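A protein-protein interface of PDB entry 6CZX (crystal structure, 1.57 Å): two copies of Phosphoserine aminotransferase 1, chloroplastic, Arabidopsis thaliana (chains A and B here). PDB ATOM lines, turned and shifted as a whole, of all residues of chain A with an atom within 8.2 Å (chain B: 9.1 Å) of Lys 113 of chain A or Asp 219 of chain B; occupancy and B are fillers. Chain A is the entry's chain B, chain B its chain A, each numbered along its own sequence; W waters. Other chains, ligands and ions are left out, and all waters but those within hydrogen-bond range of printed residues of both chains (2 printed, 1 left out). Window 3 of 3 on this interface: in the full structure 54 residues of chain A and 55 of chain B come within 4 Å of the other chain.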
ATOM      1  N   PHE A  81     -27.318 -17.169  19.595  1.00  0.00           N
ATOM      2  CA  PHE A  81     -26.320 -16.686  18.634  1.00  0.00           C
ATOM      3  C   PHE A  81     -25.736 -17.817  17.771  1.00  0.00           C
ATOM      4  O   PHE A  81     -25.371 -17.595  16.614  1.00  0.00           O
ATOM      5  CB  PHE A  81     -25.158 -15.964  19.297  1.00  0.00           C
ATOM      6  CG  PHE A  81     -25.521 -14.736  20.117  1.00  0.00           C
ATOM      7  CD1 PHE A  81     -26.726 -14.037  19.964  1.00  0.00           C
ATOM      8  CD2 PHE A  81     -24.572 -14.224  21.015  1.00  0.00           C
ATOM      9  CE1 PHE A  81     -26.990 -12.878  20.678  1.00  0.00           C
ATOM     10  CE2 PHE A  81     -24.847 -13.095  21.743  1.00  0.00           C
ATOM     11  CZ  PHE A  81     -26.068 -12.402  21.570  1.00  0.00           C
ATOM     12  N   ALA A  82     -25.602 -19.026  18.339  1.00  0.00           N
ATOM     13  CA  ALA A  82     -25.235 -20.172  17.538  1.00  0.00           C
ATOM     14  C   ALA A  82     -26.410 -20.873  16.894  1.00  0.00           C
ATOM     15  O   ALA A  82     -26.348 -21.284  15.732  1.00  0.00           O
ATOM     16  CB  ALA A  82     -24.460 -21.169  18.387  1.00  0.00           C
ATOM     17  N   PRO A  85     -27.952 -19.351  13.163  1.00  0.00           N
ATOM     18  CA  PRO A  85     -27.387 -19.784  11.862  1.00  0.00           C
ATOM     19  C   PRO A  85     -27.300 -21.293  11.678  1.00  0.00           C
ATOM     20  O   PRO A  85     -27.388 -21.782  10.567  1.00  0.00           O
ATOM     21  CB  PRO A  85     -26.005 -19.126  11.840  1.00  0.00           C
ATOM     22  CG  PRO A  85     -25.662 -18.894  13.271  1.00  0.00           C
ATOM     23  CD  PRO A  85     -26.973 -18.584  13.934  1.00  0.00           C
ATOM     24  N   LEU A  86     -27.118 -22.044  12.771  1.00  0.00           N
ATOM     25  CA  LEU A  86     -27.127 -23.508  12.690  1.00  0.00           C
ATOM     26  C   LEU A  86     -28.469 -24.030  12.125  1.00  0.00           C
ATOM     27  O   LEU A  86     -28.498 -24.932  11.262  1.00  0.00           O
ATOM     28  CB  LEU A  86     -26.840 -24.164  14.039  1.00  0.00           C
ATOM     29  CG  LEU A  86     -25.358 -24.246  14.440  1.00  0.00           C
ATOM     30  CD1 LEU A  86     -25.223 -24.616  15.907  1.00  0.00           C
ATOM     31  CD2 LEU A  86     -24.610 -25.239  13.560  1.00  0.00           C
ATOM     32  N   SER A  91     -23.809 -23.680   5.566  1.00  0.00           N
ATOM     33  CA  SER A  91     -22.499 -23.143   5.855  1.00  0.00           C
ATOM     34  C   SER A  91     -22.009 -22.070   4.877  1.00  0.00           C
ATOM     35  O   SER A  91     -21.210 -21.202   5.265  1.00  0.00           O
ATOM     36  CB  SER A  91     -21.471 -24.298   5.994  1.00  0.00           C
ATOM     37  OG  SER A  91     -21.249 -24.864   4.736  1.00  0.00           O
ATOM     38  N   ALA A 107     -23.204 -11.401  18.465  1.00  0.00           N
ATOM     39  CA  ALA A 107     -23.976 -12.250  17.540  1.00  0.00           C
ATOM     40  C   ALA A 107     -23.256 -12.482  16.226  1.00  0.00           C
ATOM     41  O   ALA A 107     -23.215 -13.613  15.741  1.00  0.00           O
ATOM     42  CB  ALA A 107     -25.368 -11.685  17.331  1.00  0.00           C
ATOM     43  N   VAL A 108     -22.627 -11.437  15.679  1.00  0.00           N
ATOM     44  CA  VAL A 108     -21.816 -11.564  14.473  1.00  0.00           C
ATOM     45  C   VAL A 108     -20.689 -12.586  14.705  1.00  0.00           C
ATOM     46  O   VAL A 108     -20.485 -13.483  13.917  1.00  0.00           O
ATOM     47  CB  VAL A 108     -21.173 -10.216  14.068  1.00  0.00           C
ATOM     48  CG1 VAL A 108     -20.140 -10.419  12.966  1.00  0.00           C
ATOM     49  CG2 VAL A 108     -22.223  -9.244  13.615  1.00  0.00           C
ATOM     50  N   LYS A 109     -19.920 -12.416  15.776  1.00  0.00           N
ATOM     51  CA  LYS A 109     -18.744 -13.248  16.033  1.00  0.00           C
ATOM     52  C   LYS A 109     -19.086 -14.733  16.105  1.00  0.00           C
ATOM     53  O   LYS A 109     -18.383 -15.582  15.568  1.00  0.00           O
ATOM     54  CB  LYS A 109     -18.071 -12.810  17.316  1.00  0.00           C
ATOM     55  CG  LYS A 109     -16.773 -13.578  17.555  1.00  0.00           C
ATOM     56  CD  LYS A 109     -15.829 -12.833  18.495  1.00  0.00           C
ATOM     57  CE  LYS A 109     -14.416 -13.414  18.442  1.00  0.00           C
ATOM     58  NZ  LYS A 109     -14.269 -14.456  19.486  1.00  0.00           N
ATOM     59  N   GLU A 110     -20.189 -15.049  16.769  1.00  0.00           N
ATOM     60  CA  GLU A 110     -20.596 -16.446  16.913  1.00  0.00           C
ATOM     61  C   GLU A 110     -21.127 -16.957  15.569  1.00  0.00           C
ATOM     62  O   GLU A 110     -20.845 -18.070  15.185  1.00  0.00           O
ATOM     63  CB  GLU A 110     -21.656 -16.576  17.986  1.00  0.00           C
ATOM     64  CG  GLU A 110     -22.102 -17.997  18.298  1.00  0.00           C
ATOM     65  CD  GLU A 110     -21.075 -18.828  19.107  1.00  0.00           C
ATOM     66  OE1 GLU A 110     -19.868 -18.463  19.234  1.00  0.00           O
ATOM     67  OE2 GLU A 110     -21.470 -19.887  19.621  1.00  0.00           O
ATOM     68  N   ALA A 111     -21.882 -16.151  14.818  1.00  0.00           N
ATOM     69  CA  ALA A 111     -22.416 -16.626  13.514  1.00  0.00           C
ATOM     70  C   ALA A 111     -21.319 -16.983  12.525  1.00  0.00           C
ATOM     71  O   ALA A 111     -21.517 -17.887  11.687  1.00  0.00           O
ATOM     72  CB  ALA A 111     -23.368 -15.600  12.879  1.00  0.00           C
ATOM     73  N   LYS A 112     -20.178 -16.308  12.603  1.00  0.00           N
ATOM     74  CA  LYS A 112     -19.030 -16.589  11.682  1.00  0.00           C
ATOM     75  C   LYS A 112     -18.595 -18.019  11.743  1.00  0.00           C
ATOM     76  O   LYS A 112     -18.054 -18.536  10.776  1.00  0.00           O
ATOM     77  CB  LYS A 112     -17.815 -15.709  12.000  1.00  0.00           C
ATOM     78  CG  LYS A 112     -18.049 -14.292  11.601  1.00  0.00           C
ATOM     79  CD  LYS A 112     -16.772 -13.471  11.766  1.00  0.00           C
ATOM     80  CE  LYS A 112     -17.036 -12.061  11.262  1.00  0.00           C
ATOM     81  NZ  LYS A 112     -15.958 -11.096  11.619  1.00  0.00           N
ATOM     82  N   LYS A 113     -18.865 -18.697  12.844  1.00  0.00           N
ATOM     83  CA  LYS A 113     -18.485 -20.109  12.952  1.00  0.00           C
ATOM     84  C   LYS A 113     -19.301 -20.985  12.030  1.00  0.00           C
ATOM     85  O   LYS A 113     -18.878 -22.079  11.695  1.00  0.00           O
ATOM     86  CB  LYS A 113     -18.670 -20.637  14.361  1.00  0.00           C
ATOM     87  CG  LYS A 113     -17.750 -20.065  15.413  1.00  0.00           C
ATOM     88  CD  LYS A 113     -18.183 -20.634  16.773  1.00  0.00           C
ATOM     89  CE  LYS A 113     -17.307 -20.157  17.883  1.00  0.00           C
ATOM     90  NZ  LYS A 113     -17.954 -20.356  19.172  1.00  0.00           N
ATOM     91  N   TYR A 114     -20.477 -20.516  11.642  1.00  0.00           N
ATOM     92  CA  TYR A 114     -21.494 -21.384  11.039  1.00  0.00           C
ATOM     93  C   TYR A 114     -21.939 -21.009   9.632  1.00  0.00           C
ATOM     94  O   TYR A 114     -22.607 -21.800   8.961  1.00  0.00           O
ATOM     95  CB  TYR A 114     -22.717 -21.467  11.956  1.00  0.00           C
ATOM     96  CG  TYR A 114     -22.318 -21.953  13.340  1.00  0.00           C
ATOM     97  CD1 TYR A 114     -21.707 -23.171  13.492  1.00  0.00           C
ATOM     98  CD2 TYR A 114     -22.447 -21.141  14.473  1.00  0.00           C
ATOM     99  CE1 TYR A 114     -21.287 -23.614  14.739  1.00  0.00           C
ATOM    100  CE2 TYR A 114     -22.009 -21.553  15.704  1.00  0.00           C
ATOM    101  CZ  TYR A 114     -21.448 -22.817  15.853  1.00  0.00           C
ATOM    102  OH  TYR A 114     -21.037 -23.223  17.117  1.00  0.00           O
ATOM    103  N   CYS A 115     -21.707 -19.768   9.247  1.00  0.00           N
ATOM    104  CA  CYS A 115     -22.060 -19.316   7.927  1.00  0.00           C
ATOM    105  C   CYS A 115     -21.278 -18.046   7.621  1.00  0.00           C
ATOM    106  O   CYS A 115     -20.424 -17.619   8.408  1.00  0.00           O
ATOM    107  CB  CYS A 115     -23.565 -19.064   7.836  1.00  0.00           C
ATOM    108  SG  CYS A 115     -24.206 -17.730   8.825  1.00  0.00           S
ATOM    109  N   LYS A 116     -21.539 -17.458   6.477  1.00  0.00           N
ATOM    110  CA  LYS A 116     -20.946 -16.171   6.130  1.00  0.00           C
ATOM    111  C   LYS A 116     -21.717 -14.982   6.697  1.00  0.00           C
ATOM    112  O   LYS A 116     -22.924 -15.000   6.752  1.00  0.00           O
ATOM    113  CB  LYS A 116     -20.888 -16.053   4.604  1.00  0.00           C
ATOM    114  CG  LYS A 116     -19.874 -17.013   3.988  1.00  0.00           C
ATOM    115  CD  LYS A 116     -19.644 -16.666   2.525  1.00  0.00           C
ATOM    116  CE  LYS A 116     -20.487 -17.559   1.672  1.00  0.00           C
ATOM    117  NZ  LYS A 116     -20.381 -17.257   0.218  1.00  0.00           N
ATOM    118  N   THR A 117     -20.995 -13.931   7.071  1.00  0.00           N
ATOM    119  CA  THR A 117     -21.602 -12.765   7.658  1.00  0.00           C
ATOM    120  C   THR A 117     -21.226 -11.522   6.878  1.00  0.00           C
ATOM    121  O   THR A 117     -20.066 -11.359   6.474  1.00  0.00           O
ATOM    122  CB  THR A 117     -21.246 -12.607   9.154  1.00  0.00           C
ATOM    123  OG1 THR A 117     -19.840 -12.345   9.343  1.00  0.00           O
ATOM    124  CG2 THR A 117     -21.643 -13.874   9.975  1.00  0.00           C
ATOM    125  N   GLN A 218     -28.333 -27.516  10.153  1.00  0.00           N
ATOM    126  CA  GLN A 218     -27.065 -28.127   9.795  1.00  0.00           C
ATOM    127  C   GLN A 218     -26.859 -29.445  10.574  1.00  0.00           C
ATOM    128  O   GLN A 218     -27.337 -29.596  11.711  1.00  0.00           O
ATOM    129  CB  GLN A 218     -25.887 -27.182  10.054  1.00  0.00           C
ATOM    130  CG  GLN A 218     -25.928 -25.939   9.213  1.00  0.00           C
ATOM    131  CD  GLN A 218     -24.689 -25.109   9.355  1.00  0.00           C
ATOM    132  OE1 GLN A 218     -23.580 -25.644   9.482  1.00  0.00           O
ATOM    133  NE2 GLN A 218     -24.877 -23.799   9.406  1.00  0.00           N
ATOM    134  N   ILE A 220     -24.380 -30.662  12.063  1.00  0.00           N
ATOM    135  CA  ILE A 220     -23.622 -30.450  13.306  1.00  0.00           C
ATOM    136  C   ILE A 220     -24.406 -29.793  14.440  1.00  0.00           C
ATOM    137  O   ILE A 220     -23.855 -29.539  15.528  1.00  0.00           O
ATOM    138  CB  ILE A 220     -22.333 -29.641  13.096  1.00  0.00           C
ATOM    139  CG1 ILE A 220     -22.626 -28.331  12.350  1.00  0.00           C
ATOM    140  CG2 ILE A 220     -21.299 -30.510  12.426  1.00  0.00           C
ATOM    141  CD1 ILE A 220     -21.575 -27.264  12.466  1.00  0.00           C
ATOM    142  N   PRO B  85     -17.910 -34.515  23.322  1.00  0.00           N
ATOM    143  CA  PRO B  85     -17.024 -34.779  22.159  1.00  0.00           C
ATOM    144  C   PRO B  85     -16.579 -33.510  21.465  1.00  0.00           C
ATOM    145  O   PRO B  85     -15.485 -33.458  20.901  1.00  0.00           O
ATOM    146  CB  PRO B  85     -17.899 -35.675  21.256  1.00  0.00           C
ATOM    147  CG  PRO B  85     -19.299 -35.332  21.665  1.00  0.00           C
ATOM    148  CD  PRO B  85     -19.237 -35.107  23.144  1.00  0.00           C
ATOM    149  N   LEU B  86     -17.399 -32.449  21.504  1.00  0.00           N
ATOM    150  CA  LEU B  86     -16.949 -31.189  20.942  1.00  0.00           C
ATOM    151  C   LEU B  86     -15.715 -30.650  21.647  1.00  0.00           C
ATOM    152  O   LEU B  86     -14.791 -30.146  20.990  1.00  0.00           O
ATOM    153  CB  LEU B  86     -18.075 -30.176  20.974  1.00  0.00           C
ATOM    154  CG  LEU B  86     -19.122 -30.284  19.850  1.00  0.00           C
ATOM    155  CD1 LEU B  86     -20.355 -29.472  20.203  1.00  0.00           C
ATOM    156  CD2 LEU B  86     -18.554 -29.844  18.491  1.00  0.00           C
ATOM    157  N   ASN B  87     -15.650 -30.794  22.970  1.00  0.00           N
ATOM    158  CA  ASN B  87     -14.514 -30.258  23.742  1.00  0.00           C
ATOM    159  C   ASN B  87     -13.326 -31.220  23.747  1.00  0.00           C
ATOM    160  O   ASN B  87     -12.169 -30.784  23.744  1.00  0.00           O
ATOM    161  CB  ASN B  87     -14.913 -29.941  25.183  1.00  0.00           C
ATOM    162  CG  ASN B  87     -15.646 -28.634  25.282  1.00  0.00           C
ATOM    163  OD1 ASN B  87     -15.012 -27.603  25.476  1.00  0.00           O
ATOM    164  ND2 ASN B  87     -16.967 -28.656  25.090  1.00  0.00           N
ATOM    165  N   CYS B  89     -12.619 -34.194  21.785  1.00  0.00           N
ATOM    166  CA  CYS B  89     -12.244 -34.989  20.608  1.00  0.00           C
ATOM    167  C   CYS B  89     -12.060 -34.141  19.405  1.00  0.00           C
ATOM    168  O   CYS B  89     -12.652 -33.065  19.314  1.00  0.00           O
ATOM    169  CB  CYS B  89     -13.341 -35.999  20.260  1.00  0.00           C
ATOM    170  SG  CYS B  89     -13.632 -37.203  21.573  1.00  0.00           S
ATOM    171  N   LYS B  90     -11.269 -34.648  18.467  1.00  0.00           N
ATOM    172  CA  LYS B  90     -11.268 -34.183  17.096  1.00  0.00           C
ATOM    173  C   LYS B  90     -12.249 -35.047  16.338  1.00  0.00           C
ATOM    174  O   LYS B  90     -12.653 -36.113  16.804  1.00  0.00           O
ATOM    175  CB  LYS B  90      -9.866 -34.304  16.474  1.00  0.00           C
ATOM    176  CG  LYS B  90      -8.836 -33.412  17.133  1.00  0.00           C
ATOM    177  CD  LYS B  90      -7.470 -33.535  16.480  1.00  0.00           C
ATOM    178  CE  LYS B  90      -6.736 -34.809  16.892  1.00  0.00           C
ATOM    179  NZ  LYS B  90      -5.254 -34.723  16.611  1.00  0.00           N
ATOM    180  N   SER B  91     -12.619 -34.593  15.149  1.00  0.00           N
ATOM    181  CA  SER B  91     -13.675 -35.233  14.391  1.00  0.00           C
ATOM    182  C   SER B  91     -13.397 -36.689  14.041  1.00  0.00           C
ATOM    183  O   SER B  91     -14.338 -37.439  13.822  1.00  0.00           O
ATOM    184  CB  SER B  91     -13.981 -34.416  13.127  1.00  0.00           C
ATOM    185  OG  SER B  91     -12.861 -34.405  12.294  1.00  0.00           O
ATOM    186  N   ASN B 216      -8.919 -26.457  23.694  1.00  0.00           N
ATOM    187  CA  ASN B 216      -8.836 -27.093  22.390  1.00  0.00           C
ATOM    188  C   ASN B 216     -10.127 -27.781  21.934  1.00  0.00           C
ATOM    189  O   ASN B 216     -10.074 -28.825  21.289  1.00  0.00           O
ATOM    190  CB  ASN B 216      -7.703 -28.134  22.373  1.00  0.00           C
ATOM    191  CG  ASN B 216      -6.349 -27.541  22.719  1.00  0.00           C
ATOM    192  OD1 ASN B 216      -5.656 -28.056  23.617  1.00  0.00           O
ATOM    193  ND2 ASN B 216      -5.947 -26.451  22.008  1.00  0.00           N
ATOM    194  N   ALA B 217     -11.272 -27.173  22.213  1.00  0.00           N
ATOM    195  CA  ALA B 217     -12.529 -27.645  21.635  1.00  0.00           C
ATOM    196  C   ALA B 217     -12.512 -27.503  20.095  1.00  0.00           C
ATOM    197  O   ALA B 217     -11.744 -26.726  19.501  1.00  0.00           O
ATOM    198  CB  ALA B 217     -13.705 -26.861  22.185  1.00  0.00           C
ATOM    199  N   GLN B 218     -13.360 -28.271  19.434  1.00  0.00           N
ATOM    200  CA  GLN B 218     -13.495 -28.139  17.994  1.00  0.00           C
ATOM    201  C   GLN B 218     -13.952 -26.732  17.603  1.00  0.00           C
ATOM    202  O   GLN B 218     -14.664 -26.095  18.339  1.00  0.00           O
ATOM    203  CB  GLN B 218     -14.478 -29.174  17.459  1.00  0.00           C
ATOM    204  CG  GLN B 218     -14.012 -30.613  17.665  1.00  0.00           C
ATOM    205  CD  GLN B 218     -14.922 -31.642  16.975  1.00  0.00           C
ATOM    206  OE1 GLN B 218     -15.475 -31.375  15.887  1.00  0.00           O
ATOM    207  NE2 GLN B 218     -15.113 -32.799  17.612  1.00  0.00           N
ATOM    208  N   ASP B 219     -13.535 -26.259  16.427  1.00  0.00           N
ATOM    209  CA  ASP B 219     -13.890 -24.904  16.007  1.00  0.00           C
ATOM    210  C   ASP B 219     -15.386 -24.635  15.919  1.00  0.00           C
ATOM    211  O   ASP B 219     -15.827 -23.494  16.090  1.00  0.00           O
ATOM    212  CB  ASP B 219     -13.260 -24.564  14.654  1.00  0.00           C
ATOM    213  CG  ASP B 219     -11.756 -24.315  14.742  1.00  0.00           C
ATOM    214  OD1 ASP B 219     -11.165 -24.237  15.865  1.00  0.00           O
ATOM    215  OD2 ASP B 219     -11.154 -24.169  13.651  1.00  0.00           O
ATOM    216  N   ILE B 220     -16.163 -25.667  15.640  1.00  0.00           N
ATOM    217  CA  ILE B 220     -17.614 -25.526  15.520  1.00  0.00           C
ATOM    218  C   ILE B 220     -18.330 -25.531  16.877  1.00  0.00           C
ATOM    219  O   ILE B 220     -19.556 -25.413  16.947  1.00  0.00           O
ATOM    220  CB  ILE B 220     -18.234 -26.648  14.642  1.00  0.00           C
ATOM    221  CG1 ILE B 220     -17.760 -28.033  15.137  1.00  0.00           C
ATOM    222  CG2 ILE B 220     -17.922 -26.431  13.151  1.00  0.00           C
ATOM    223  CD1 ILE B 220     -18.725 -29.151  14.805  1.00  0.00           C
ATOM    224  N   THR B 221     -17.576 -25.652  17.967  1.00  0.00           N
ATOM    225  CA  THR B 221     -18.217 -25.628  19.292  1.00  0.00           C
ATOM    226  C   THR B 221     -18.886 -24.275  19.566  1.00  0.00           C
ATOM    227  O   THR B 221     -18.228 -23.250  19.507  1.00  0.00           O
ATOM    228  CB  THR B 221     -17.211 -25.927  20.384  1.00  0.00           C
ATOM    229  OG1 THR B 221     -16.547 -27.168  20.079  1.00  0.00           O
ATOM    230  CG2 THR B 221     -17.867 -26.024  21.733  1.00  0.00           C
ATOM    231  N   PRO B 222     -20.199 -24.284  19.868  1.00  0.00           N
ATOM    232  CA  PRO B 222     -20.793 -23.001  20.308  1.00  0.00           C
ATOM    233  C   PRO B 222     -20.051 -22.459  21.515  1.00  0.00           C
ATOM    234  O   PRO B 222     -19.604 -23.247  22.362  1.00  0.00           O
ATOM    235  CB  PRO B 222     -22.207 -23.374  20.691  1.00  0.00           C
ATOM    236  CG  PRO B 222     -22.515 -24.542  19.836  1.00  0.00           C
ATOM    237  CD  PRO B 222     -21.228 -25.337  19.782  1.00  0.00           C
ATOM    238  N   VAL B 223     -19.947 -21.141  21.634  1.00  0.00           N
ATOM    239  CA  VAL B 223     -19.244 -20.578  22.794  1.00  0.00           C
ATOM    240  C   VAL B 223     -19.919 -21.071  24.085  1.00  0.00           C
ATOM    241  O   VAL B 223     -19.240 -21.401  25.067  1.00  0.00           O
ATOM    242  CB  VAL B 223     -19.180 -19.032  22.720  1.00  0.00           C
ATOM    243  CG1 VAL B 223     -20.552 -18.368  22.911  1.00  0.00           C
ATOM    244  CG2 VAL B 223     -18.201 -18.484  23.740  1.00  0.00           C
ATOM    245  N   MET B 224     -21.244 -21.243  24.070  1.00  0.00           N
ATOM    246  CA  MET B 224     -21.962 -21.696  25.257  1.00  0.00           C
ATOM    247  C   MET B 224     -21.739 -23.185  25.612  1.00  0.00           C
ATOM    248  O   MET B 224     -22.189 -23.642  26.651  1.00  0.00           O
ATOM    249  CB  MET B 224     -23.455 -21.417  25.122  1.00  0.00           C
ATOM    250  CG  MET B 224     -23.769 -19.953  25.329  1.00  0.00           C
ATOM    251  SD  MET B 224     -23.229 -19.254  26.892  1.00  0.00           S
ATOM    252  CE  MET B 224     -24.105 -20.373  28.007  1.00  0.00           C
ATOM    253  N   LEU B 225     -21.114 -23.945  24.725  1.00  0.00           N
ATOM    254  CA  LEU B 225     -20.750 -25.334  25.016  1.00  0.00           C
ATOM    255  C   LEU B 225     -19.257 -25.516  25.310  1.00  0.00           C
ATOM    256  O   LEU B 225     -18.805 -26.631  25.497  1.00  0.00           O
ATOM    257  CB  LEU B 225     -21.219 -26.269  23.887  1.00  0.00           C
ATOM    258  CG  LEU B 225     -22.657 -26.764  24.008  1.00  0.00           C
ATOM    259  CD1 LEU B 225     -23.698 -25.650  23.914  1.00  0.00           C
ATOM    260  CD2 LEU B 225     -22.908 -27.773  22.916  1.00  0.00           C
ATOM    261  N   ASP B 226     -18.493 -24.429  25.329  1.00  0.00           N
ATOM    262  CA  ASP B 226     -17.030 -24.477  25.402  1.00  0.00           C
ATOM    263  C   ASP B 226     -16.541 -24.477  26.847  1.00  0.00           C
ATOM    264  O   ASP B 226     -16.760 -23.524  27.567  1.00  0.00           O
ATOM    265  CB  ASP B 226     -16.472 -23.269  24.642  1.00  0.00           C
ATOM    266  CG  ASP B 226     -14.951 -23.293  24.506  1.00  0.00           C
ATOM    267  OD1 ASP B 226     -14.257 -23.276  25.527  1.00  0.00           O
ATOM    268  OD2 ASP B 226     -14.484 -23.246  23.371  1.00  0.00           O
ATOM    269  N   ILE B 229     -14.189 -21.579  28.034  1.00  0.00           N
ATOM    270  CA  ILE B 229     -14.942 -20.337  28.231  1.00  0.00           C
ATOM    271  C   ILE B 229     -15.604 -20.346  29.598  1.00  0.00           C
ATOM    272  O   ILE B 229     -15.468 -19.401  30.386  1.00  0.00           O
ATOM    273  CB  ILE B 229     -16.002 -20.151  27.122  1.00  0.00           C
ATOM    274  CG1 ILE B 229     -15.327 -19.849  25.797  1.00  0.00           C
ATOM    275  CG2 ILE B 229     -17.026 -19.071  27.469  1.00  0.00           C
ATOM    276  CD1 ILE B 229     -14.753 -18.457  25.688  1.00  0.00           C
ATOM    277  N   TYR B 237     -19.760 -16.598  32.164  1.00  0.00           N
ATOM    278  CA  TYR B 237     -19.490 -16.008  30.852  1.00  0.00           C
ATOM    279  C   TYR B 237     -20.718 -15.253  30.372  1.00  0.00           C
ATOM    280  O   TYR B 237     -20.627 -14.101  29.945  1.00  0.00           O
ATOM    281  CB  TYR B 237     -19.089 -17.064  29.831  1.00  0.00           C
ATOM    282  CG  TYR B 237     -18.929 -16.474  28.453  1.00  0.00           C
ATOM    283  CD1 TYR B 237     -17.878 -15.622  28.158  1.00  0.00           C
ATOM    284  CD2 TYR B 237     -19.865 -16.727  27.456  1.00  0.00           C
ATOM    285  CE1 TYR B 237     -17.730 -15.045  26.887  1.00  0.00           C
ATOM    286  CE2 TYR B 237     -19.744 -16.178  26.193  1.00  0.00           C
ATOM    287  CZ  TYR B 237     -18.669 -15.340  25.909  1.00  0.00           C
ATOM    288  OH  TYR B 237     -18.513 -14.775  24.666  1.00  0.00           O
HETATM  289  O   HOH W   1     -23.309 -20.231  21.912  1.00  0.00           O
HETATM  290  O   HOH W   2     -22.160 -27.254  16.769  1.00  0.00           O
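OH of Tyr 114 of chain A is in hydrogen-bond range of O of Ile 220 of chain B (2.6 Å).
NZ of Lys 113 of chain A lies within hydrogen-bond range of O of Thr 221 of chain B, 2.9 Å away.
The side-chain carboxylate (OE2) of Glu 110 of chain A sits at hydrogen-bond distance from the backbone NH (N) of Val 223 of chain B, at 2.8 Å.
N of Val 223 of chain B sits close to NZ of Lys 113 of chain A (3.3 Å).
The side-chain hydroxyl of Tyr 114 of chain A lies close to the backbone nitrogen of Pro 222 of chain B (3.1 Å).
OG1 of Thr 221 of chain B lies within hydrogen-bond range of O of Gln 218 of chain B (2.8 Å).
NZ of Lys 113 of chain A lies within salt-bridge range of OE1 of Glu 110 of chain A, 2.7 Å away.
NE2 of Gln 218 of chain A sits at hydrogen-bond distance from O of Tyr 114 of chain A (3.1 Å).
Pro 222 of chain B touches Ala 82 of chain A (CB to CB, 3.9 Å).
OE2 of Glu 110 of chain A touches CA of Pro 222 of chain B, 3.3 Å away.
Lys 113 of chain A touches Asp 219 of chain B (CD to O, 3.8 Å).
Pro 222 of chain B touches Lys 113 of chain A (C to NZ, 3.8 Å).
Tyr 114 of chain A touches Thr 221 of chain B.
Ile 220 of chain A touches Ile 220 of chain B (CG2 to CD1, 3.8 Å).
Printed residues of chain B within 4 Å of Glu 110 of chain A: Pro 222 and Val 223.
Lys 113 of chain A touches four residues of chain B.
Of chain B, only Ile 220, Thr 221 and Pro 222 come within 4 Å of Tyr 114 of chain A.
Asp 219 of chain B touches just one residue of chain A: Lys 113 (3.8 Å).
Printed residues of chain A within 4 Å of Ile 220 of chain B: Tyr 114 (2.6 Å) and Ile 220 (3.8 Å).
Of the printed residues of chain A, Thr 221 of chain B touches Lys 113 and Tyr 114.
Printed residues of chain A within 4 Å of Pro 222 of chain B: Ala 82 (3.9 Å), Glu 110 (3.3 Å), Lys 113 (3.8 Å) and Tyr 114 (3.1 Å).
Of the printed residues of chain A, Val 223 of chain B touches Glu 110 (2.8 Å) and Lys 113 (3.3 Å).
Of the 18 printed residues of chain A, 5 touch a printed residue of chain B.
Printed residues of chain B that touch a printed residue of chain A: Asp 219, Ile 220, Thr 221, Pro 222 and Val 223.
Hydrophobic or aromatic side chains of chain B within 4 Å of the printed part of chain A: Ile 220, Pro 222 and Val 223.
Among the printed residues, no Asp or Glu carboxylate lies within 4 Å of a Lys or Arg side-chain nitrogen of the other chain.
Ile 220 of chain A touches its own counterpart, Ile 220 of chain B.
Positions printed for both chains: 85, 86, 91, 218 and 220.
Water W1 lies within hydrogen-bond range of the side-chain carboxylate (OE2) of Glu 110 of chain A (3.0 Å), the backbone NH (N) of Met 224 of chain B (3.2 Å) and the backbone NH (N) of Val 223 of chain B (3.5 Å).
Water W2 lies within hydrogen-bond range of the backbone carbonyl oxygen of Ile 220 of chain A (3.1 Å) and the backbone carbonyl oxygen of Ile 220 of chain B (3.2 Å).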
